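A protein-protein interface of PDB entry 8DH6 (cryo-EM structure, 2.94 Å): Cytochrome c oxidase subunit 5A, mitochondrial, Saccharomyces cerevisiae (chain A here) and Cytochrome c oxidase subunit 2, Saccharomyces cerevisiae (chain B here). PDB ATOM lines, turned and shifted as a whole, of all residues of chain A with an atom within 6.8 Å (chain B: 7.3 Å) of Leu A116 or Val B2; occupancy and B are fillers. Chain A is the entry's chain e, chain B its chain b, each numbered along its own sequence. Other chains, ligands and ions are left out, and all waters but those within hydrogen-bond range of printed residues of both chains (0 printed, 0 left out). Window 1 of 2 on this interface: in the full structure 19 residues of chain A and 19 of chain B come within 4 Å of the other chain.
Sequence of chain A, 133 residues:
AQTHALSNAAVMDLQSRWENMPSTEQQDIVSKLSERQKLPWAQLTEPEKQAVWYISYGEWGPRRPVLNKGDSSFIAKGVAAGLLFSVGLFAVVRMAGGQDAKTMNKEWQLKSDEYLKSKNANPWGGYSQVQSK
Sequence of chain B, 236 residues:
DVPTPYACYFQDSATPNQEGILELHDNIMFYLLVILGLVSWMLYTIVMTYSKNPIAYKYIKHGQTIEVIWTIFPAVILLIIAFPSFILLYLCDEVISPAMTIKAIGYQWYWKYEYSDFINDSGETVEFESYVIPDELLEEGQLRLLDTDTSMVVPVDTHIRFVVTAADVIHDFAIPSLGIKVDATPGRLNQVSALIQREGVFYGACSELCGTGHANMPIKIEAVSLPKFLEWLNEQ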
ATOM      1  N   LYS A 111      -9.298 -18.828   7.388  1.00  0.00           N
ATOM      2  CA  LYS A 111     -10.524 -18.322   6.778  1.00  0.00           C
ATOM      3  C   LYS A 111     -11.413 -19.454   6.280  1.00  0.00           C
ATOM      4  O   LYS A 111     -12.643 -19.375   6.395  1.00  0.00           O
ATOM      5  CB  LYS A 111     -10.185 -17.367   5.636  1.00  0.00           C
ATOM      6  CG  LYS A 111      -9.555 -16.069   6.101  1.00  0.00           C
ATOM      7  CD  LYS A 111      -9.296 -15.131   4.940  1.00  0.00           C
ATOM      8  CE  LYS A 111      -8.605 -13.864   5.405  1.00  0.00           C
ATOM      9  NZ  LYS A 111      -9.489 -13.032   6.268  1.00  0.00           N
ATOM     10  N   SER A 112     -10.816 -20.507   5.721  1.00  0.00           N
ATOM     11  CA  SER A 112     -11.605 -21.673   5.331  1.00  0.00           C
ATOM     12  C   SER A 112     -12.278 -22.310   6.542  1.00  0.00           C
ATOM     13  O   SER A 112     -13.444 -22.721   6.470  1.00  0.00           O
ATOM     14  CB  SER A 112     -10.722 -22.687   4.609  1.00  0.00           C
ATOM     15  OG  SER A 112     -11.477 -23.812   4.201  1.00  0.00           O
ATOM     16  N   ASP A 113     -11.560 -22.398   7.663  1.00  0.00           N
ATOM     17  CA  ASP A 113     -12.150 -22.905   8.895  1.00  0.00           C
ATOM     18  C   ASP A 113     -13.290 -22.019   9.373  1.00  0.00           C
ATOM     19  O   ASP A 113     -14.298 -22.528   9.869  1.00  0.00           O
ATOM     20  CB  ASP A 113     -11.087 -23.016   9.986  1.00  0.00           C
ATOM     21  CG  ASP A 113     -10.180 -24.209   9.795  1.00  0.00           C
ATOM     22  OD1 ASP A 113     -10.269 -24.859   8.734  1.00  0.00           O
ATOM     23  OD2 ASP A 113      -9.382 -24.499  10.709  1.00  0.00           O
ATOM     24  N   GLU A 114     -13.141 -20.698   9.255  1.00  0.00           N
ATOM     25  CA  GLU A 114     -14.223 -19.796   9.640  1.00  0.00           C
ATOM     26  C   GLU A 114     -15.456 -20.011   8.771  1.00  0.00           C
ATOM     27  O   GLU A 114     -16.586 -20.035   9.279  1.00  0.00           O
ATOM     28  CB  GLU A 114     -13.752 -18.346   9.554  1.00  0.00           C
ATOM     29  CG  GLU A 114     -14.795 -17.329   9.980  1.00  0.00           C
ATOM     30  CD  GLU A 114     -15.142 -17.423  11.453  1.00  0.00           C
ATOM     31  OE1 GLU A 114     -14.288 -17.879  12.243  1.00  0.00           O
ATOM     32  OE2 GLU A 114     -16.271 -17.040  11.824  1.00  0.00           O
ATOM     33  N   TYR A 115     -15.259 -20.175   7.461  1.00  0.00           N
ATOM     34  CA  TYR A 115     -16.392 -20.447   6.580  1.00  0.00           C
ATOM     35  C   TYR A 115     -17.068 -21.764   6.937  1.00  0.00           C
ATOM     36  O   TYR A 115     -18.301 -21.853   6.946  1.00  0.00           O
ATOM     37  CB  TYR A 115     -15.950 -20.470   5.119  1.00  0.00           C
ATOM     38  CG  TYR A 115     -16.998 -21.060   4.203  1.00  0.00           C
ATOM     39  CD1 TYR A 115     -18.168 -20.367   3.922  1.00  0.00           C
ATOM     40  CD2 TYR A 115     -16.826 -22.310   3.627  1.00  0.00           C
ATOM     41  CE1 TYR A 115     -19.133 -20.900   3.092  1.00  0.00           C
ATOM     42  CE2 TYR A 115     -17.786 -22.853   2.796  1.00  0.00           C
ATOM     43  CZ  TYR A 115     -18.937 -22.142   2.531  1.00  0.00           C
ATOM     44  OH  TYR A 115     -19.898 -22.672   1.703  1.00  0.00           O
ATOM     45  N   LEU A 116     -16.278 -22.802   7.221  1.00  0.00           N
ATOM     46  CA  LEU A 116     -16.860 -24.084   7.604  1.00  0.00           C
ATOM     47  C   LEU A 116     -17.585 -23.997   8.940  1.00  0.00           C
ATOM     48  O   LEU A 116     -18.604 -24.668   9.137  1.00  0.00           O
ATOM     49  CB  LEU A 116     -15.777 -25.157   7.656  1.00  0.00           C
ATOM     50  CG  LEU A 116     -15.189 -25.567   6.309  1.00  0.00           C
ATOM     51  CD1 LEU A 116     -14.025 -26.508   6.514  1.00  0.00           C
ATOM     52  CD2 LEU A 116     -16.254 -26.217   5.450  1.00  0.00           C
ATOM     53  N   LYS A 117     -17.073 -23.187   9.869  1.00  0.00           N
ATOM     54  CA  LYS A 117     -17.765 -22.962  11.132  1.00  0.00           C
ATOM     55  C   LYS A 117     -19.082 -22.231  10.917  1.00  0.00           C
ATOM     56  O   LYS A 117     -20.041 -22.448  11.665  1.00  0.00           O
ATOM     57  CB  LYS A 117     -16.867 -22.177  12.086  1.00  0.00           C
ATOM     58  CG  LYS A 117     -17.457 -21.960  13.467  1.00  0.00           C
ATOM     59  CD  LYS A 117     -16.481 -21.220  14.368  1.00  0.00           C
ATOM     60  CE  LYS A 117     -17.024 -21.080  15.780  1.00  0.00           C
ATOM     61  NZ  LYS A 117     -18.209 -20.179  15.835  1.00  0.00           N
ATOM     62  N   SER A 118     -19.144 -21.362   9.905  1.00  0.00           N
ATOM     63  CA  SER A 118     -20.411 -20.726   9.559  1.00  0.00           C
ATOM     64  C   SER A 118     -21.445 -21.755   9.117  1.00  0.00           C
ATOM     65  O   SER A 118     -22.627 -21.641   9.456  1.00  0.00           O
ATOM     66  CB  SER A 118     -20.192 -19.685   8.466  1.00  0.00           C
ATOM     67  OG  SER A 118     -21.414 -19.076   8.090  1.00  0.00           O
ATOM     68  N   LYS A 119     -21.020 -22.768   8.365  1.00  0.00           N
ATOM     69  CA  LYS A 119     -21.920 -23.775   7.820  1.00  0.00           C
ATOM     70  C   LYS A 119     -22.181 -24.934   8.773  1.00  0.00           C
ATOM     71  O   LYS A 119     -22.921 -25.853   8.408  1.00  0.00           O
ATOM     72  CB  LYS A 119     -21.362 -24.328   6.505  1.00  0.00           C
ATOM     73  CG  LYS A 119     -21.160 -23.316   5.379  1.00  0.00           C
ATOM     74  CD  LYS A 119     -22.461 -22.799   4.770  1.00  0.00           C
ATOM     75  CE  LYS A 119     -22.931 -21.503   5.410  1.00  0.00           C
ATOM     76  NZ  LYS A 119     -24.138 -20.955   4.735  1.00  0.00           N
ATOM     77  N   ASN A 120     -21.595 -24.916   9.973  1.00  0.00           N
ATOM     78  CA  ASN A 120     -21.714 -26.016  10.926  1.00  0.00           C
ATOM     79  C   ASN A 120     -21.287 -27.338  10.303  1.00  0.00           C
ATOM     80  O   ASN A 120     -21.968 -28.355  10.469  1.00  0.00           O
ATOM     81  CB  ASN A 120     -23.145 -26.129  11.462  1.00  0.00           C
ATOM     82  CG  ASN A 120     -23.547 -24.943  12.314  1.00  0.00           C
ATOM     83  OD1 ASN A 120     -22.929 -24.665  13.339  1.00  0.00           O
ATOM     84  ND2 ASN A 120     -24.596 -24.244  11.897  1.00  0.00           N
ATOM     85  N   ALA A 121     -20.173 -27.331   9.578  1.00  0.00           N
ATOM     86  CA  ALA A 121     -19.670 -28.541   8.949  1.00  0.00           C
ATOM     87  C   ALA A 121     -18.900 -29.390   9.951  1.00  0.00           C
ATOM     88  O   ALA A 121     -18.137 -28.878  10.774  1.00  0.00           O
ATOM     89  CB  ALA A 121     -18.771 -28.197   7.762  1.00  0.00           C
ATOM     90  N   ASN A 122     -19.105 -30.708   9.863  1.00  0.00           N
ATOM     91  CA  ASN A 122     -18.501 -31.696  10.752  1.00  0.00           C
ATOM     92  C   ASN A 122     -18.729 -31.316  12.212  1.00  0.00           C
ATOM     93  O   ASN A 122     -17.781 -30.926  12.904  1.00  0.00           O
ATOM     94  CB  ASN A 122     -17.005 -31.840  10.468  1.00  0.00           C
ATOM     95  CG  ASN A 122     -16.727 -32.594   9.185  1.00  0.00           C
ATOM     96  OD1 ASN A 122     -17.401 -33.571   8.867  1.00  0.00           O
ATOM     97  ND2 ASN A 122     -15.721 -32.148   8.443  1.00  0.00           N
ATOM     98  N   GLY A 126     -14.257 -33.278  13.082  1.00  0.00           N
ATOM     99  CA  GLY A 126     -13.418 -32.102  12.980  1.00  0.00           C
ATOM    100  C   GLY A 126     -13.477 -31.441  11.619  1.00  0.00           C
ATOM    101  O   GLY A 126     -13.276 -32.100  10.595  1.00  0.00           O
ATOM    102  N   TYR A 127     -13.755 -30.141  11.591  1.00  0.00           N
ATOM    103  CA  TYR A 127     -13.768 -29.384  10.349  1.00  0.00           C
ATOM    104  C   TYR A 127     -12.527 -28.527  10.168  1.00  0.00           C
ATOM    105  O   TYR A 127     -12.342 -27.951   9.091  1.00  0.00           O
ATOM    106  CB  TYR A 127     -15.013 -28.495  10.276  1.00  0.00           C
ATOM    107  CG  TYR A 127     -15.034 -27.371  11.287  1.00  0.00           C
ATOM    108  CD1 TYR A 127     -15.569 -27.561  12.551  1.00  0.00           C
ATOM    109  CD2 TYR A 127     -14.520 -26.120  10.976  1.00  0.00           C
ATOM    110  CE1 TYR A 127     -15.590 -26.539  13.477  1.00  0.00           C
ATOM    111  CE2 TYR A 127     -14.535 -25.094  11.895  1.00  0.00           C
ATOM    112  CZ  TYR A 127     -15.072 -25.308  13.145  1.00  0.00           C
ATOM    113  OH  TYR A 127     -15.092 -24.288  14.065  1.00  0.00           O
ATOM    114  N   SER A 128     -11.676 -28.426  11.185  1.00  0.00           N
ATOM    115  CA  SER A 128     -10.522 -27.542  11.124  1.00  0.00           C
ATOM    116  C   SER A 128      -9.505 -28.093  10.134  1.00  0.00           C
ATOM    117  O   SER A 128      -9.079 -29.247  10.246  1.00  0.00           O
ATOM    118  CB  SER A 128      -9.891 -27.382  12.505  1.00  0.00           C
ATOM    119  OG  SER A 128      -8.648 -26.711  12.411  1.00  0.00           O
ATOM    120  N   GLN A 129      -9.125 -27.268   9.168  1.00  0.00           N
ATOM    121  CA  GLN A 129      -8.125 -27.612   8.167  1.00  0.00           C
ATOM    122  C   GLN A 129      -7.011 -26.581   8.266  1.00  0.00           C
ATOM    123  O   GLN A 129      -7.157 -25.467   7.761  1.00  0.00           O
ATOM    124  CB  GLN A 129      -8.732 -27.611   6.768  1.00  0.00           C
ATOM    125  CG  GLN A 129      -9.892 -28.566   6.582  1.00  0.00           C
ATOM    126  CD  GLN A 129     -10.395 -28.578   5.158  1.00  0.00           C
ATOM    127  OE1 GLN A 129      -9.899 -27.840   4.308  1.00  0.00           O
ATOM    128  NE2 GLN A 129     -11.382 -29.418   4.888  1.00  0.00           N
ATOM    129  N   ASP B   1     -18.609 -34.039   6.370  1.00  0.00           N
ATOM    130  CA  ASP B   1     -19.088 -33.020   5.443  1.00  0.00           C
ATOM    131  C   ASP B   1     -17.978 -32.603   4.492  1.00  0.00           C
ATOM    132  O   ASP B   1     -18.162 -32.576   3.277  1.00  0.00           O
ATOM    133  CB  ASP B   1     -19.613 -31.806   6.207  1.00  0.00           C
ATOM    134  CG  ASP B   1     -20.721 -32.164   7.172  1.00  0.00           C
ATOM    135  OD1 ASP B   1     -21.390 -33.193   6.949  1.00  0.00           O
ATOM    136  OD2 ASP B   1     -20.927 -31.422   8.153  1.00  0.00           O
ATOM    137  N   VAL B   2     -16.822 -32.281   5.062  1.00  0.00           N
ATOM    138  CA  VAL B   2     -15.658 -31.847   4.296  1.00  0.00           C
ATOM    139  C   VAL B   2     -14.451 -32.622   4.814  1.00  0.00           C
ATOM    140  O   VAL B   2     -14.360 -32.877   6.024  1.00  0.00           O
ATOM    141  CB  VAL B   2     -15.473 -30.324   4.402  1.00  0.00           C
ATOM    142  CG1 VAL B   2     -15.199 -29.909   5.836  1.00  0.00           C
ATOM    143  CG2 VAL B   2     -14.374 -29.839   3.487  1.00  0.00           C
ATOM    144  N   PRO B   3     -13.528 -33.050   3.954  1.00  0.00           N
ATOM    145  CA  PRO B   3     -12.358 -33.787   4.441  1.00  0.00           C
ATOM    146  C   PRO B   3     -11.486 -32.944   5.358  1.00  0.00           C
ATOM    147  O   PRO B   3     -11.369 -31.726   5.207  1.00  0.00           O
ATOM    148  CB  PRO B   3     -11.612 -34.160   3.154  1.00  0.00           C
ATOM    149  CG  PRO B   3     -12.135 -33.221   2.122  1.00  0.00           C
ATOM    150  CD  PRO B   3     -13.569 -33.025   2.484  1.00  0.00           C
ATOM    151  N   THR B   4     -10.870 -33.622   6.325  1.00  0.00           N
ATOM    152  CA  THR B   4     -10.013 -33.058   7.352  1.00  0.00           C
ATOM    153  C   THR B   4      -8.599 -33.609   7.215  1.00  0.00           C
ATOM    154  O   THR B   4      -8.429 -34.802   6.940  1.00  0.00           O
ATOM    155  CB  THR B   4     -10.558 -33.392   8.746  1.00  0.00           C
ATOM    156  OG1 THR B   4     -11.967 -33.145   8.775  1.00  0.00           O
ATOM    157  CG2 THR B   4      -9.890 -32.544   9.813  1.00  0.00           C
ATOM    158  N   PRO B   5      -7.571 -32.775   7.373  1.00  0.00           N
ATOM    159  CA  PRO B   5      -6.197 -33.275   7.249  1.00  0.00           C
ATOM    160  C   PRO B   5      -5.878 -34.345   8.281  1.00  0.00           C
ATOM    161  O   PRO B   5      -6.308 -34.271   9.434  1.00  0.00           O
ATOM    162  CB  PRO B   5      -5.342 -32.020   7.466  1.00  0.00           C
ATOM    163  CG  PRO B   5      -6.258 -31.030   8.113  1.00  0.00           C
ATOM    164  CD  PRO B   5      -7.598 -31.314   7.532  1.00  0.00           C
ATOM    165  N   ALA B   7      -6.884 -37.337   8.631  1.00  0.00           N
ATOM    166  CA  ALA B   7      -8.044 -38.053   9.133  1.00  0.00           C
ATOM    167  C   ALA B   7      -7.971 -39.526   8.750  1.00  0.00           C
ATOM    168  O   ALA B   7      -7.448 -39.896   7.697  1.00  0.00           O
ATOM    169  CB  ALA B   7      -9.336 -37.439   8.601  1.00  0.00           C
ATOM    170  N   GLN B  11     -16.197 -39.237   7.048  1.00  0.00           N
ATOM    171  CA  GLN B  11     -16.706 -37.904   7.313  1.00  0.00           C
ATOM    172  C   GLN B  11     -18.008 -38.000   8.102  1.00  0.00           C
ATOM    173  O   GLN B  11     -18.676 -39.038   8.128  1.00  0.00           O
ATOM    174  CB  GLN B  11     -16.915 -37.137   6.010  1.00  0.00           C
ATOM    175  CG  GLN B  11     -15.799 -37.322   5.003  1.00  0.00           C
ATOM    176  CD  GLN B  11     -15.934 -36.403   3.810  1.00  0.00           C
ATOM    177  OE1 GLN B  11     -16.797 -35.528   3.782  1.00  0.00           O
ATOM    178  NE2 GLN B  11     -15.075 -36.592   2.817  1.00  0.00           N
ATOM    179  N   ASP B  12     -18.364 -36.904   8.763  1.00  0.00           N
ATOM    180  CA  ASP B  12     -19.550 -36.901   9.607  1.00  0.00           C
ATOM    181  C   ASP B  12     -20.798 -37.153   8.770  1.00  0.00           C
ATOM    182  O   ASP B  12     -20.989 -36.542   7.715  1.00  0.00           O
ATOM    183  CB  ASP B  12     -19.662 -35.578  10.358  1.00  0.00           C
ATOM    184  CG  ASP B  12     -18.737 -35.514  11.552  1.00  0.00           C
ATOM    185  OD1 ASP B  12     -18.046 -36.518  11.814  1.00  0.00           O
ATOM    186  OD2 ASP B  12     -18.708 -34.472  12.237  1.00  0.00           O
ATOM    187  N   GLY B 141     -10.105 -18.181   1.247  1.00  0.00           N
ATOM    188  CA  GLY B 141     -11.049 -18.801   2.154  1.00  0.00           C
ATOM    189  C   GLY B 141     -11.757 -19.993   1.546  1.00  0.00           C
ATOM    190  O   GLY B 141     -12.115 -20.940   2.251  1.00  0.00           O
ATOM    191  N   LEU B 143     -12.349 -23.430  -0.725  1.00  0.00           N
ATOM    192  CA  LEU B 143     -11.602 -24.680  -0.765  1.00  0.00           C
ATOM    193  C   LEU B 143     -11.201 -25.002  -2.200  1.00  0.00           C
ATOM    194  O   LEU B 143     -12.046 -25.007  -3.100  1.00  0.00           O
ATOM    195  CB  LEU B 143     -12.433 -25.813  -0.168  1.00  0.00           C
ATOM    196  CG  LEU B 143     -12.656 -25.744   1.343  1.00  0.00           C
ATOM    197  CD1 LEU B 143     -13.978 -25.070   1.667  1.00  0.00           C
ATOM    198  CD2 LEU B 143     -12.593 -27.121   1.960  1.00  0.00           C
ATOM    199  N   LEU B 146     -12.671 -28.074  -4.534  1.00  0.00           N
ATOM    200  CA  LEU B 146     -13.796 -28.591  -3.764  1.00  0.00           C
ATOM    201  C   LEU B 146     -15.009 -27.677  -3.749  1.00  0.00           C
ATOM    202  O   LEU B 146     -16.121 -28.176  -3.552  1.00  0.00           O
ATOM    203  CB  LEU B 146     -13.355 -28.868  -2.321  1.00  0.00           C
ATOM    204  CG  LEU B 146     -14.126 -29.900  -1.506  1.00  0.00           C
ATOM    205  CD1 LEU B 146     -14.073 -31.251  -2.191  1.00  0.00           C
ATOM    206  CD2 LEU B 146     -13.527 -29.998  -0.121  1.00  0.00           C
ATOM    207  N   SER B 177     -20.255 -37.839   2.621  1.00  0.00           N
ATOM    208  CA  SER B 177     -20.919 -37.423   3.850  1.00  0.00           C
ATOM    209  C   SER B 177     -22.392 -37.805   3.858  1.00  0.00           C
ATOM    210  O   SER B 177     -22.923 -38.178   4.908  1.00  0.00           O
ATOM    211  CB  SER B 177     -20.767 -35.917   4.046  1.00  0.00           C
ATOM    212  OG  SER B 177     -21.435 -35.495   5.220  1.00  0.00           O
ATOM    213  N   ARG B 198     -29.305 -32.778   8.873  1.00  0.00           N
ATOM    214  CA  ARG B 198     -28.797 -31.541   9.443  1.00  0.00           C
ATOM    215  C   ARG B 198     -28.384 -30.602   8.322  1.00  0.00           C
ATOM    216  O   ARG B 198     -27.870 -31.033   7.288  1.00  0.00           O
ATOM    217  CB  ARG B 198     -27.612 -31.798  10.377  1.00  0.00           C
ATOM    218  CG  ARG B 198     -26.486 -32.581   9.736  1.00  0.00           C
ATOM    219  CD  ARG B 198     -25.355 -32.823  10.710  1.00  0.00           C
ATOM    220  NE  ARG B 198     -24.318 -33.661  10.126  1.00  0.00           N
ATOM    221  CZ  ARG B 198     -23.283 -33.198   9.440  1.00  0.00           C
ATOM    222  NH1 ARG B 198     -23.115 -31.903   9.234  1.00  0.00           N
ATOM    223  NH2 ARG B 198     -22.395 -34.057   8.948  1.00  0.00           N
ATOM    224  N   VAL B 201     -23.129 -27.900   4.602  1.00  0.00           N
ATOM    225  CA  VAL B 201     -22.561 -28.103   3.278  1.00  0.00           C
ATOM    226  C   VAL B 201     -21.919 -29.481   3.232  1.00  0.00           C
ATOM    227  O   VAL B 201     -21.411 -29.988   4.237  1.00  0.00           O
ATOM    228  CB  VAL B 201     -21.545 -26.997   2.915  1.00  0.00           C
ATOM    229  CG1 VAL B 201     -20.237 -27.198   3.660  1.00  0.00           C
ATOM    230  CG2 VAL B 201     -21.320 -26.956   1.418  1.00  0.00           C
ATOM    231  N   PHE B 202     -21.972 -30.103   2.057  1.00  0.00           N
ATOM    232  CA  PHE B 202     -21.481 -31.461   1.868  1.00  0.00           C
ATOM    233  C   PHE B 202     -20.737 -31.520   0.546  1.00  0.00           C
ATOM    234  O   PHE B 202     -21.303 -31.199  -0.504  1.00  0.00           O
ATOM    235  CB  PHE B 202     -22.634 -32.468   1.890  1.00  0.00           C
ATOM    236  CG  PHE B 202     -23.563 -32.292   3.055  1.00  0.00           C
ATOM    237  CD1 PHE B 202     -23.197 -32.715   4.318  1.00  0.00           C
ATOM    238  CD2 PHE B 202     -24.796 -31.688   2.890  1.00  0.00           C
ATOM    239  CE1 PHE B 202     -24.046 -32.547   5.391  1.00  0.00           C
ATOM    240  CE2 PHE B 202     -25.649 -31.518   3.959  1.00  0.00           C
ATOM    241  CZ  PHE B 202     -25.273 -31.948   5.212  1.00  0.00           C
ATOM    242  N   TYR B 203     -19.476 -31.925   0.600  1.00  0.00           N
ATOM    243  CA  TYR B 203     -18.630 -31.947  -0.578  1.00  0.00           C
ATOM    244  C   TYR B 203     -18.347 -33.379  -1.010  1.00  0.00           C
ATOM    245  O   TYR B 203     -18.121 -34.268  -0.185  1.00  0.00           O
ATOM    246  CB  TYR B 203     -17.313 -31.220  -0.311  1.00  0.00           C
ATOM    247  CG  TYR B 203     -17.471 -29.743  -0.050  1.00  0.00           C
ATOM    248  CD1 TYR B 203     -17.697 -28.860  -1.089  1.00  0.00           C
ATOM    249  CD2 TYR B 203     -17.375 -29.231   1.234  1.00  0.00           C
ATOM    250  CE1 TYR B 203     -17.834 -27.511  -0.859  1.00  0.00           C
ATOM    251  CE2 TYR B 203     -17.510 -27.884   1.473  1.00  0.00           C
ATOM    252  CZ  TYR B 203     -17.741 -27.027   0.424  1.00  0.00           C
ATOM    253  OH  TYR B 203     -17.878 -25.680   0.654  1.00  0.00           O
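Of the 16 printed residues of chain A, 10 touch a printed residue of chain B. Along chain A the printed residues that touch a printed residue of chain B span positions 111 to 129. Printed residues of chain B that touch a printed residue of chain A: Asp B1, Val B2, Pro B3, Thr B4, Pro B5, Asp B12, Gly B141, Leu B143, Arg B198 and Tyr B203. Along chain B the printed residues that touch a printed residue of chain A span positions 1 to 203. Among the printed residues, no Asp or Glu carboxylate lies within 4 Å of a Lys or Arg side-chain nitrogen of the other chain.
The backbone NH of Asn A122 is in hydrogen-bond range of the side-chain carboxylate of Asp B1 (2.6 Å). The backbone carbonyl oxygen (O) of Pro B3 sits close to the side-chain amide nitrogen (NE2) of Gln A129. The backbone carbonyl oxygen of Val B2 lies within hydrogen-bond range of the side-chain amide nitrogen of Asn A122 (2.9 Å). The backbone carbonyl oxygen of Gly A126 sits at hydrogen-bond distance from the side-chain hydroxyl of Thr B4. The side-chain amide oxygen (OD1) of Asn A122 sits close to the backbone NH (N) of Asp B12.
Printed residues of chain B within 4 Å of Ser A112: Gly B141 and Leu B143. Of chain B, only Val B2 (3.7 Å) comes within 4 Å of Leu A116. Printed residues of chain B within 4 Å of Asn A122: Asp B1, Val B2, Thr B4 and Asp B12. Tyr A127 touches none of the printed residues of chain B. Of the printed residues of chain A, Asp B1 touches Asn A120, Ala A121 and Asn A122. Of chain A, only Leu A116 (3.7 Å), Asn A122 (2.9 Å) and Gln A129 (3.3 Å) come within 4 Å of Val B2. Gln B11 touches none of the printed residues of chain A. Of the printed residues of chain A, Asp B12 touches Asn A122 (3.2 Å). Printed residues of chain A within 4 Å of Leu B143: Ser A112 (3.6 Å) and Gln A129 (3.6 Å). The nearest printed residue of chain B that does not touch Leu A116 is Val B201 (4.5 Å). The nearest residue of chain A that does not touch Val B2 is Ala A121 (4.4 Å).
The side-chain amide oxygen of Gln B11 lies close to the backbone carbonyl oxygen of Asp B1 (3.3 Å). OD1 of Asp A113 is in hydrogen-bond range of N of Gln A129 (2.7 Å). The backbone carbonyl oxygen of Asp B1 lies within hydrogen-bond range of the backbone NH of Tyr B203, 3.1 Å away. The side-chain carboxylate (OD2) of Asp A113 sits at hydrogen-bond distance from the side-chain hydroxyl (OG) of Ser A128, 2.9 Å away. The backbone NH (N) of Val B2 is in hydrogen-bond range of the side-chain amide oxygen (OE1) of Gln B11, at 3.5 Å. O of Leu A116 lies within hydrogen-bond range of N of Ala A121, 3.1 Å away.
Among the printed residues, pairs that only touch across the chains: Lys A111 with Gly B141 (3.9 Å), Ser A112 with Gly B141 (3.2 Å), Ser A112 with Leu B143 (3.6 Å), Tyr A115 with Tyr B203 (3.5 Å), Leu A116 with Val B2 (3.7 Å), Asn A120 with Asp B1 (3.98 Å), Asn A120 with Arg B198 (3.9 Å), Ala A121 with Asp B1 (3.2 Å), Asn A122 with Thr B4 (3.9 Å), Ser A128 with Thr B4 (3.4 Å), Ser A128 with Pro B5 (3.7 Å), Gln A129 with Val B2 (3.3 Å), Gln A129 with Pro B5 (3.7 Å) and Gln A129 with Leu B143 (3.6 Å).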
